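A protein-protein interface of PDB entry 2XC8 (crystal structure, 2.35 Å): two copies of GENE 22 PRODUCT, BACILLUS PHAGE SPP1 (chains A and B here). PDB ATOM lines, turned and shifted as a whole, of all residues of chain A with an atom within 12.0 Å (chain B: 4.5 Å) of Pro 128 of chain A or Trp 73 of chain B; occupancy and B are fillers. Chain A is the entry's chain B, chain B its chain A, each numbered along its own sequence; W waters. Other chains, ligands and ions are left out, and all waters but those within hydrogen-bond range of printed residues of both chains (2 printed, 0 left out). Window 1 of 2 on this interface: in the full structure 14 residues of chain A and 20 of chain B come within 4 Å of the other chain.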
ATOM      1  N   ILE A   4     -10.284   3.426   1.308  1.00  0.00           N
ATOM      2  CA  ILE A   4      -8.917   3.646   0.850  1.00  0.00           C
ATOM      3  C   ILE A   4      -8.211   2.316   0.591  1.00  0.00           C
ATOM      4  O   ILE A   4      -8.219   1.416   1.441  1.00  0.00           O
ATOM      5  CB  ILE A   4      -8.123   4.561   1.819  1.00  0.00           C
ATOM      6  CG1 ILE A   4      -8.645   5.999   1.691  1.00  0.00           C
ATOM      7  CG2 ILE A   4      -6.618   4.483   1.544  1.00  0.00           C
ATOM      8  CD1 ILE A   4      -7.946   7.028   2.565  1.00  0.00           C
ATOM      9  N   GLU A  16      -0.952  13.283  -1.959  1.00  0.00           N
ATOM     10  CA  GLU A  16      -1.931  13.036  -0.957  1.00  0.00           C
ATOM     11  C   GLU A  16      -3.320  13.162  -1.561  1.00  0.00           C
ATOM     12  O   GLU A  16      -3.626  14.144  -2.141  1.00  0.00           O
ATOM     13  CB  GLU A  16      -1.756  14.101   0.085  1.00  0.00           C
ATOM     14  CG  GLU A  16      -2.245  13.805   1.402  1.00  0.00           C
ATOM     15  CD  GLU A  16      -1.878  14.900   2.372  1.00  0.00           C
ATOM     16  OE1 GLU A  16      -2.716  15.745   2.596  1.00  0.00           O
ATOM     17  OE2 GLU A  16      -0.769  14.927   2.919  1.00  0.00           O
ATOM     18  N   LYS A  18      -7.370  12.880  -0.591  1.00  0.00           N
ATOM     19  CA  LYS A  18      -8.356  12.826   0.478  1.00  0.00           C
ATOM     20  C   LYS A  18      -9.779  13.311   0.197  1.00  0.00           C
ATOM     21  O   LYS A  18     -10.009  14.187  -0.593  1.00  0.00           O
ATOM     22  CB  LYS A  18      -7.821  13.496   1.751  1.00  0.00           C
ATOM     23  CG  LYS A  18      -7.767  14.958   1.700  1.00  0.00           C
ATOM     24  CD  LYS A  18      -7.447  15.493   3.008  1.00  0.00           C
ATOM     25  CE  LYS A  18      -6.067  15.998   3.045  1.00  0.00           C
ATOM     26  NZ  LYS A  18      -6.034  17.389   3.524  1.00  0.00           N
ATOM     27  N   LYS A 126       6.021   8.513   7.358  1.00  0.00           N
ATOM     28  CA  LYS A 126       5.065   7.957   8.313  1.00  0.00           C
ATOM     29  C   LYS A 126       5.544   7.695   9.747  1.00  0.00           C
ATOM     30  O   LYS A 126       4.706   7.522  10.627  1.00  0.00           O
ATOM     31  CB  LYS A 126       4.600   6.569   7.868  1.00  0.00           C
ATOM     32  N   PRO A 127       6.880   7.662   9.985  1.00  0.00           N
ATOM     33  CA  PRO A 127       7.396   7.483  11.337  1.00  0.00           C
ATOM     34  C   PRO A 127       6.746   8.648  12.072  1.00  0.00           C
ATOM     35  O   PRO A 127       6.857   9.796  11.628  1.00  0.00           O
ATOM     36  CB  PRO A 127       8.897   7.624  11.069  1.00  0.00           C
ATOM     37  CG  PRO A 127       9.106   6.934   9.744  1.00  0.00           C
ATOM     38  CD  PRO A 127       7.760   6.802   9.057  1.00  0.00           C
ATOM     39  N   PRO A 128       6.047   8.349  13.184  1.00  0.00           N
ATOM     40  CA  PRO A 128       5.456   9.430  13.945  1.00  0.00           C
ATOM     41  C   PRO A 128       6.572   9.785  14.904  1.00  0.00           C
ATOM     42  O   PRO A 128       7.345   8.904  15.307  1.00  0.00           O
ATOM     43  CB  PRO A 128       4.283   8.793  14.706  1.00  0.00           C
ATOM     44  CG  PRO A 128       4.263   7.338  14.337  1.00  0.00           C
ATOM     45  CD  PRO A 128       5.480   7.032  13.541  1.00  0.00           C
ATOM     46  N   VAL A 129       6.677  11.049  15.237  1.00  0.00           N
ATOM     47  CA  VAL A 129       7.640  11.455  16.213  1.00  0.00           C
ATOM     48  C   VAL A 129       7.486  10.528  17.436  1.00  0.00           C
ATOM     49  O   VAL A 129       6.433  10.032  17.696  1.00  0.00           O
ATOM     50  CB  VAL A 129       7.454  12.931  16.508  1.00  0.00           C
ATOM     51  CG1 VAL A 129       8.612  13.485  17.224  1.00  0.00           C
ATOM     52  CG2 VAL A 129       7.330  13.675  15.219  1.00  0.00           C
ATOM     53  N   ILE A 130       8.552  10.247  18.154  1.00  0.00           N
ATOM     54  CA  ILE A 130       8.414   9.492  19.358  1.00  0.00           C
ATOM     55  C   ILE A 130       8.127  10.409  20.510  1.00  0.00           C
ATOM     56  O   ILE A 130       8.956  11.196  20.830  1.00  0.00           O
ATOM     57  CB  ILE A 130       9.685   8.776  19.671  1.00  0.00           C
ATOM     58  CG1 ILE A 130       9.523   7.930  20.915  1.00  0.00           C
ATOM     59  CG2 ILE A 130      10.768   9.757  19.956  1.00  0.00           C
ATOM     60  CD1 ILE A 130       9.004   6.569  20.694  1.00  0.00           C
ATOM     61  N   VAL A 131       6.942  10.285  21.153  1.00  0.00           N
ATOM     62  CA  VAL A 131       6.591  10.981  22.427  1.00  0.00           C
ATOM     63  C   VAL A 131       7.096   9.997  23.434  1.00  0.00           C
ATOM     64  O   VAL A 131       6.368   9.117  23.905  1.00  0.00           O
ATOM     65  CB  VAL A 131       5.045  11.311  22.704  1.00  0.00           C
ATOM     66  CG1 VAL A 131       4.584  10.718  24.024  1.00  0.00           C
ATOM     67  CG2 VAL A 131       4.825  12.849  22.915  1.00  0.00           C
ATOM     68  N   GLU A 132       8.365  10.145  23.767  1.00  0.00           N
ATOM     69  CA  GLU A 132       8.940   9.222  24.707  1.00  0.00           C
ATOM     70  C   GLU A 132       9.992   9.821  25.597  1.00  0.00           C
ATOM     71  O   GLU A 132      11.162   9.714  25.271  1.00  0.00           O
ATOM     72  CB  GLU A 132       9.549   8.150  23.816  1.00  0.00           C
ATOM     73  N   LEU B  13     -12.009  12.892  13.124  1.00  0.00           N
ATOM     74  CA  LEU B  13     -10.959  12.673  12.139  1.00  0.00           C
ATOM     75  C   LEU B  13     -11.467  11.804  10.990  1.00  0.00           C
ATOM     76  O   LEU B  13     -12.004  10.716  11.215  1.00  0.00           O
ATOM     77  CB  LEU B  13      -9.748  12.021  12.818  1.00  0.00           C
ATOM     78  CG  LEU B  13      -8.461  11.765  12.031  1.00  0.00           C
ATOM     79  CD1 LEU B  13      -7.788  13.067  11.617  1.00  0.00           C
ATOM     80  CD2 LEU B  13      -7.505  10.908  12.848  1.00  0.00           C
ATOM     81  N   VAL B  26      -2.540   4.669   9.161  1.00  0.00           N
ATOM     82  CA  VAL B  26      -3.460   5.801   9.204  1.00  0.00           C
ATOM     83  C   VAL B  26      -3.306   6.588   7.909  1.00  0.00           C
ATOM     84  O   VAL B  26      -2.206   7.025   7.565  1.00  0.00           O
ATOM     85  CB  VAL B  26      -3.197   6.723  10.424  1.00  0.00           C
ATOM     86  CG1 VAL B  26      -4.207   7.867  10.468  1.00  0.00           C
ATOM     87  CG2 VAL B  26      -3.241   5.929  11.724  1.00  0.00           C
ATOM     88  N   VAL B  41      -4.364  16.555   8.149  1.00  0.00           N
ATOM     89  CA  VAL B  41      -3.650  15.541   8.925  1.00  0.00           C
ATOM     90  C   VAL B  41      -2.902  14.596   7.987  1.00  0.00           C
ATOM     91  O   VAL B  41      -3.497  13.996   7.087  1.00  0.00           O
ATOM     92  CB  VAL B  41      -4.608  14.749   9.859  1.00  0.00           C
ATOM     93  CG1 VAL B  41      -3.864  13.641  10.589  1.00  0.00           C
ATOM     94  CG2 VAL B  41      -5.269  15.682  10.864  1.00  0.00           C
ATOM     95  N   GLU B  42      -1.594  14.481   8.205  1.00  0.00           N
ATOM     96  CA  GLU B  42      -0.724  13.631   7.393  1.00  0.00           C
ATOM     97  C   GLU B  42      -0.968  12.152   7.669  1.00  0.00           C
ATOM     98  O   GLU B  42      -1.495  11.786   8.725  1.00  0.00           O
ATOM     99  CB  GLU B  42       0.749  13.948   7.672  1.00  0.00           C
ATOM    100  CG  GLU B  42       1.165  15.391   7.427  1.00  0.00           C
ATOM    101  CD  GLU B  42       2.596  15.659   7.864  1.00  0.00           C
ATOM    102  OE1 GLU B  42       2.878  15.568   9.080  1.00  0.00           O
ATOM    103  OE2 GLU B  42       3.437  15.971   6.991  1.00  0.00           O
ATOM    104  N   GLU B  43      -0.610  11.300   6.751  1.00  0.00           N
ATOM    105  CA  GLU B  43      -0.666   9.887   6.948  1.00  0.00           C
ATOM    106  C   GLU B  43       0.425   9.440   7.935  1.00  0.00           C
ATOM    107  O   GLU B  43       1.350  10.126   8.163  1.00  0.00           O
ATOM    108  CB  GLU B  43      -0.597   9.193   5.599  1.00  0.00           C
ATOM    109  CG  GLU B  43       0.638   8.472   5.385  1.00  0.00           C
ATOM    110  CD  GLU B  43       1.208   8.627   4.023  1.00  0.00           C
ATOM    111  OE1 GLU B  43       0.910   7.805   3.159  1.00  0.00           O
ATOM    112  OE2 GLU B  43       1.994   9.554   3.815  1.00  0.00           O
ATOM    113  N   VAL B  44       0.234   8.311   8.570  1.00  0.00           N
ATOM    114  CA  VAL B  44       1.163   7.784   9.563  1.00  0.00           C
ATOM    115  C   VAL B  44       1.007   6.264   9.642  1.00  0.00           C
ATOM    116  O   VAL B  44      -0.088   5.735   9.438  1.00  0.00           O
ATOM    117  CB  VAL B  44       0.952   8.471  10.951  1.00  0.00           C
ATOM    118  CG1 VAL B  44       0.126   7.610  11.904  1.00  0.00           C
ATOM    119  CG2 VAL B  44       2.274   8.825  11.580  1.00  0.00           C
ATOM    120  N   SER B  45       2.108   5.567   9.911  1.00  0.00           N
ATOM    121  CA  SER B  45       2.089   4.113  10.061  1.00  0.00           C
ATOM    122  C   SER B  45       3.204   3.636  10.986  1.00  0.00           C
ATOM    123  O   SER B  45       4.261   4.269  11.072  1.00  0.00           O
ATOM    124  CB  SER B  45       2.187   3.412   8.699  1.00  0.00           C
ATOM    125  OG  SER B  45       3.483   3.535   8.139  1.00  0.00           O
ATOM    126  N   LEU B  60      -0.953   6.079  20.121  1.00  0.00           N
ATOM    127  CA  LEU B  60      -0.765   7.079  19.078  1.00  0.00           C
ATOM    128  C   LEU B  60      -1.505   8.363  19.442  1.00  0.00           C
ATOM    129  O   LEU B  60      -2.704   8.336  19.718  1.00  0.00           O
ATOM    130  CB  LEU B  60      -1.258   6.524  17.735  1.00  0.00           C
ATOM    131  CG  LEU B  60      -1.080   7.334  16.447  1.00  0.00           C
ATOM    132  CD1 LEU B  60       0.389   7.450  16.049  1.00  0.00           C
ATOM    133  CD2 LEU B  60      -1.884   6.702  15.322  1.00  0.00           C
ATOM    134  N   TYR B  61      -0.765   9.459  19.495  1.00  0.00           N
ATOM    135  CA  TYR B  61      -1.259  10.769  19.835  1.00  0.00           C
ATOM    136  C   TYR B  61      -1.397  11.775  18.688  1.00  0.00           C
ATOM    137  O   TYR B  61      -0.550  11.910  17.881  1.00  0.00           O
ATOM    138  CB  TYR B  61      -0.417  11.431  20.928  1.00  0.00           C
ATOM    139  CG  TYR B  61      -0.142  10.623  22.135  1.00  0.00           C
ATOM    140  CD1 TYR B  61      -1.130  10.333  23.037  1.00  0.00           C
ATOM    141  CD2 TYR B  61       1.125  10.149  22.386  1.00  0.00           C
ATOM    142  CE1 TYR B  61      -0.881   9.617  24.101  1.00  0.00           C
ATOM    143  CE2 TYR B  61       1.383   9.428  23.459  1.00  0.00           C
ATOM    144  CZ  TYR B  61       0.382   9.156  24.313  1.00  0.00           C
ATOM    145  OH  TYR B  61       0.633   8.429  25.391  1.00  0.00           O
ATOM    146  N   LEU B  62      -2.519  12.461  18.666  1.00  0.00           N
ATOM    147  CA  LEU B  62      -2.784  13.500  17.738  1.00  0.00           C
ATOM    148  C   LEU B  62      -2.902  14.823  18.468  1.00  0.00           C
ATOM    149  O   LEU B  62      -3.828  15.088  19.153  1.00  0.00           O
ATOM    150  CB  LEU B  62      -4.013  13.224  16.922  1.00  0.00           C
ATOM    151  CG  LEU B  62      -4.216  14.164  15.741  1.00  0.00           C
ATOM    152  CD1 LEU B  62      -3.378  13.865  14.539  1.00  0.00           C
ATOM    153  CD2 LEU B  62      -5.628  14.219  15.400  1.00  0.00           C
ATOM    154  N   HIS B  63      -1.920  15.666  18.261  1.00  0.00           N
ATOM    155  CA  HIS B  63      -1.791  16.924  18.996  1.00  0.00           C
ATOM    156  C   HIS B  63      -1.572  18.106  18.054  1.00  0.00           C
ATOM    157  O   HIS B  63      -1.167  17.925  16.904  1.00  0.00           O
ATOM    158  CB  HIS B  63      -0.653  16.833  20.015  1.00  0.00           C
ATOM    159  CG  HIS B  63       0.614  16.274  19.451  1.00  0.00           C
ATOM    160  ND1 HIS B  63       1.544  17.051  18.797  1.00  0.00           N
ATOM    161  CD2 HIS B  63       1.098  15.010  19.429  1.00  0.00           C
ATOM    162  CE1 HIS B  63       2.550  16.293  18.401  1.00  0.00           C
ATOM    163  NE2 HIS B  63       2.303  15.049  18.771  1.00  0.00           N
ATOM    164  N   SER B  72      -0.052  17.215  14.448  1.00  0.00           N
ATOM    165  CA  SER B  72       0.995  16.207  14.271  1.00  0.00           C
ATOM    166  C   SER B  72       0.729  14.898  15.016  1.00  0.00           C
ATOM    167  O   SER B  72      -0.103  14.841  15.925  1.00  0.00           O
ATOM    168  CB  SER B  72       2.353  16.777  14.691  1.00  0.00           C
ATOM    169  OG  SER B  72       2.684  17.927  13.934  1.00  0.00           O
ATOM    170  N   TRP B  73       1.454  13.855  14.613  1.00  0.00           N
ATOM    171  CA  TRP B  73       1.382  12.548  15.254  1.00  0.00           C
ATOM    172  C   TRP B  73       2.559  12.311  16.190  1.00  0.00           C
ATOM    173  O   TRP B  73       3.691  12.723  15.911  1.00  0.00           O
ATOM    174  CB  TRP B  73       1.356  11.428  14.213  1.00  0.00           C
ATOM    175  CG  TRP B  73       0.133  11.388  13.354  1.00  0.00           C
ATOM    176  CD1 TRP B  73       0.050  11.736  12.038  1.00  0.00           C
ATOM    177  CD2 TRP B  73      -1.181  10.959  13.740  1.00  0.00           C
ATOM    178  NE1 TRP B  73      -1.232  11.556  11.579  1.00  0.00           N
ATOM    179  CE2 TRP B  73      -2.009  11.082  12.602  1.00  0.00           C
ATOM    180  CE3 TRP B  73      -1.741  10.489  14.936  1.00  0.00           C
ATOM    181  CZ2 TRP B  73      -3.367  10.748  12.623  1.00  0.00           C
ATOM    182  CZ3 TRP B  73      -3.094  10.159  14.957  1.00  0.00           C
ATOM    183  CH2 TRP B  73      -3.891  10.291  13.806  1.00  0.00           C
ATOM    184  N   SER B  74       2.272  11.639  17.298  1.00  0.00           N
ATOM    185  CA  SER B  74       3.287  11.162  18.219  1.00  0.00           C
ATOM    186  C   SER B  74       2.965   9.732  18.614  1.00  0.00           C
ATOM    187  O   SER B  74       1.796   9.368  18.753  1.00  0.00           O
ATOM    188  CB  SER B  74       3.349  12.046  19.457  1.00  0.00           C
ATOM    189  OG  SER B  74       4.070  13.235  19.188  1.00  0.00           O
ATOM    190  N   LEU B  75       4.002   8.920  18.787  1.00  0.00           N
ATOM    191  CA  LEU B  75       3.817   7.534  19.186  1.00  0.00           C
ATOM    192  C   LEU B  75       4.583   7.222  20.461  1.00  0.00           C
ATOM    193  O   LEU B  75       5.790   7.456  20.549  1.00  0.00           O
ATOM    194  CB  LEU B  75       4.237   6.581  18.059  1.00  0.00           C
ATOM    195  CG  LEU B  75       4.083   5.072  18.290  1.00  0.00           C
ATOM    196  CD1 LEU B  75       2.620   4.639  18.247  1.00  0.00           C
ATOM    197  CD2 LEU B  75       4.897   4.294  17.267  1.00  0.00           C
ATOM    198  N   PRO B  98      -6.357   8.005  19.056  1.00  0.00           N
ATOM    199  CA  PRO B  98      -7.218   7.074  18.319  1.00  0.00           C
ATOM    200  C   PRO B  98      -6.748   5.616  18.301  1.00  0.00           C
ATOM    201  O   PRO B  98      -7.527   4.735  17.936  1.00  0.00           O
ATOM    202  CB  PRO B  98      -7.218   7.650  16.900  1.00  0.00           C
ATOM    203  CG  PRO B  98      -5.922   8.354  16.782  1.00  0.00           C
ATOM    204  CD  PRO B  98      -5.625   8.908  18.146  1.00  0.00           C
HETATM  205  O   HOH W   1      -3.814  15.932   5.097  1.00  0.00           O
HETATM  206  O   HOH W   2       0.205  12.475   4.340  1.00  0.00           O
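N of Val 129 of chain A sits at hydrogen-bond distance from O of Trp 73 of chain B, 3.5 Å away. N of Leu 75 of chain B lies within hydrogen-bond range of O of Val 129 of chain A (2.9 Å). O of Lys 126 of chain A is in hydrogen-bond range of N of Ser 45 of chain B (3.3 Å). The backbone carbonyl oxygen of Leu 75 of chain B is in hydrogen-bond range of the backbone NH of Val 131 of chain A, 3.1 Å away.
The backbone carbonyl oxygen (O) of Glu 42 of chain B lies within hydrogen-bond range of the indole nitrogen (NE1) of Trp 73 of chain B (2.9 Å). A ring nitrogen (NE2) of His 63 of chain B sits at hydrogen-bond distance from the side-chain hydroxyl (OG) of Ser 74 of chain B, 2.6 Å away. The backbone carbonyl oxygen (O) of Ser 74 of chain B lies within hydrogen-bond range of the backbone NH (N) of Tyr 61 of chain B (2.7 Å). The backbone NH (N) of Val 26 of chain B sits at hydrogen-bond distance from the backbone carbonyl oxygen (O) of Val 44 of chain B, 2.7 Å away.
Lys 126 of chain A touches Val 44 of chain B. Pro 128 of chain A touches Val 44 of chain B. Pro 128 of chain A touches Ser 45 of chain B. Trp 73 of chain B touches Pro 128 of chain A (CB to CB, 3.97 Å). Pro 128 of chain A touches Leu 75 of chain B. O of Val 129 of chain A touches CA of Ser 74 of chain B, at 3.4 Å. CD1 of Ile 130 of chain A touches O of Leu 75 of chain B, at 3.3 Å. Val 131 of chain A touches Tyr 61 of chain B (CG1 to CE2, 3.5 Å). Ser 74 of chain B touches Val 131 of chain A (CB to CB, 3.7 Å).
Of the printed residues of chain B, Lys 126 of chain A touches Val 44 and Ser 45. Pro 128 of chain A touches four residues of chain B. Of the printed residues of chain B, Val 129 of chain A touches Trp 73 (3.5 Å), Ser 74 (3.4 Å) and Leu 75 (2.9 Å). Printed residues of chain B within 4 Å of Ile 130 of chain A: Leu 75. Printed residues of chain B within 4 Å of Val 131 of chain A: Tyr 61 (3.5 Å), Ser 74 (3.7 Å) and Leu 75 (3.1 Å). No residue of chain A comes within 4 Å of Val 26 of chain B. No residue of chain A comes within 4 Å of Val 41 of chain B. Glu 43 of chain B touches none of the printed residues of chain A. Of chain A, only Lys 126 (2.9 Å) and Pro 128 (3.7 Å) come within 4 Å of Val 44 of chain B. No residue of chain A comes within 4 Å of Leu 62 of chain B. No residue of chain A comes within 4 Å of Ser 72 of chain B. Trp 73 of chain B touches just these residues of chain A: Pro 128 (3.97 Å) and Val 129 (3.5 Å). Ser 74 of chain B touches just these residues of chain A: Val 129 (3.4 Å) and Val 131 (3.7 Å). No residue of chain A comes within 4 Å of Pro 98 of chain B. The nearest printed residue of chain B that does not touch Pro 128 of chain A is Ser 74 of chain B (4.2 Å).
Hydrophobic or aromatic side chains of chain A within 4 Å of the printed part of chain B: Pro 128, Val 129, Ile 130 and Val 131. Along chain B the printed residues that touch a printed residue of chain A span positions 44 to 75. Among the printed residues, no Asp or Glu carboxylate lies within 4 Å of a Lys or Arg side-chain nitrogen of the other chain.
No position is printed for both chains. Of the 13 pairs that touch across the chains among the printed residues, none has its exchanged pair printed and touching as well.
Water W1 lies within hydrogen-bond range of the side-chain carboxylate (OE1) of Glu 16 of chain A (2.7 Å), the backbone carbonyl oxygen (O) of Val 41 of chain B (2.8 Å) and the side-chain amino group (NZ) of Lys 18 of chain A (3.1 Å). Water W2 bridges the backbone NH (N) of Glu 43 of chain B (2.8 Å) and the side-chain carboxylate (OE2) of Glu 16 of chain A (3.0 Å).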
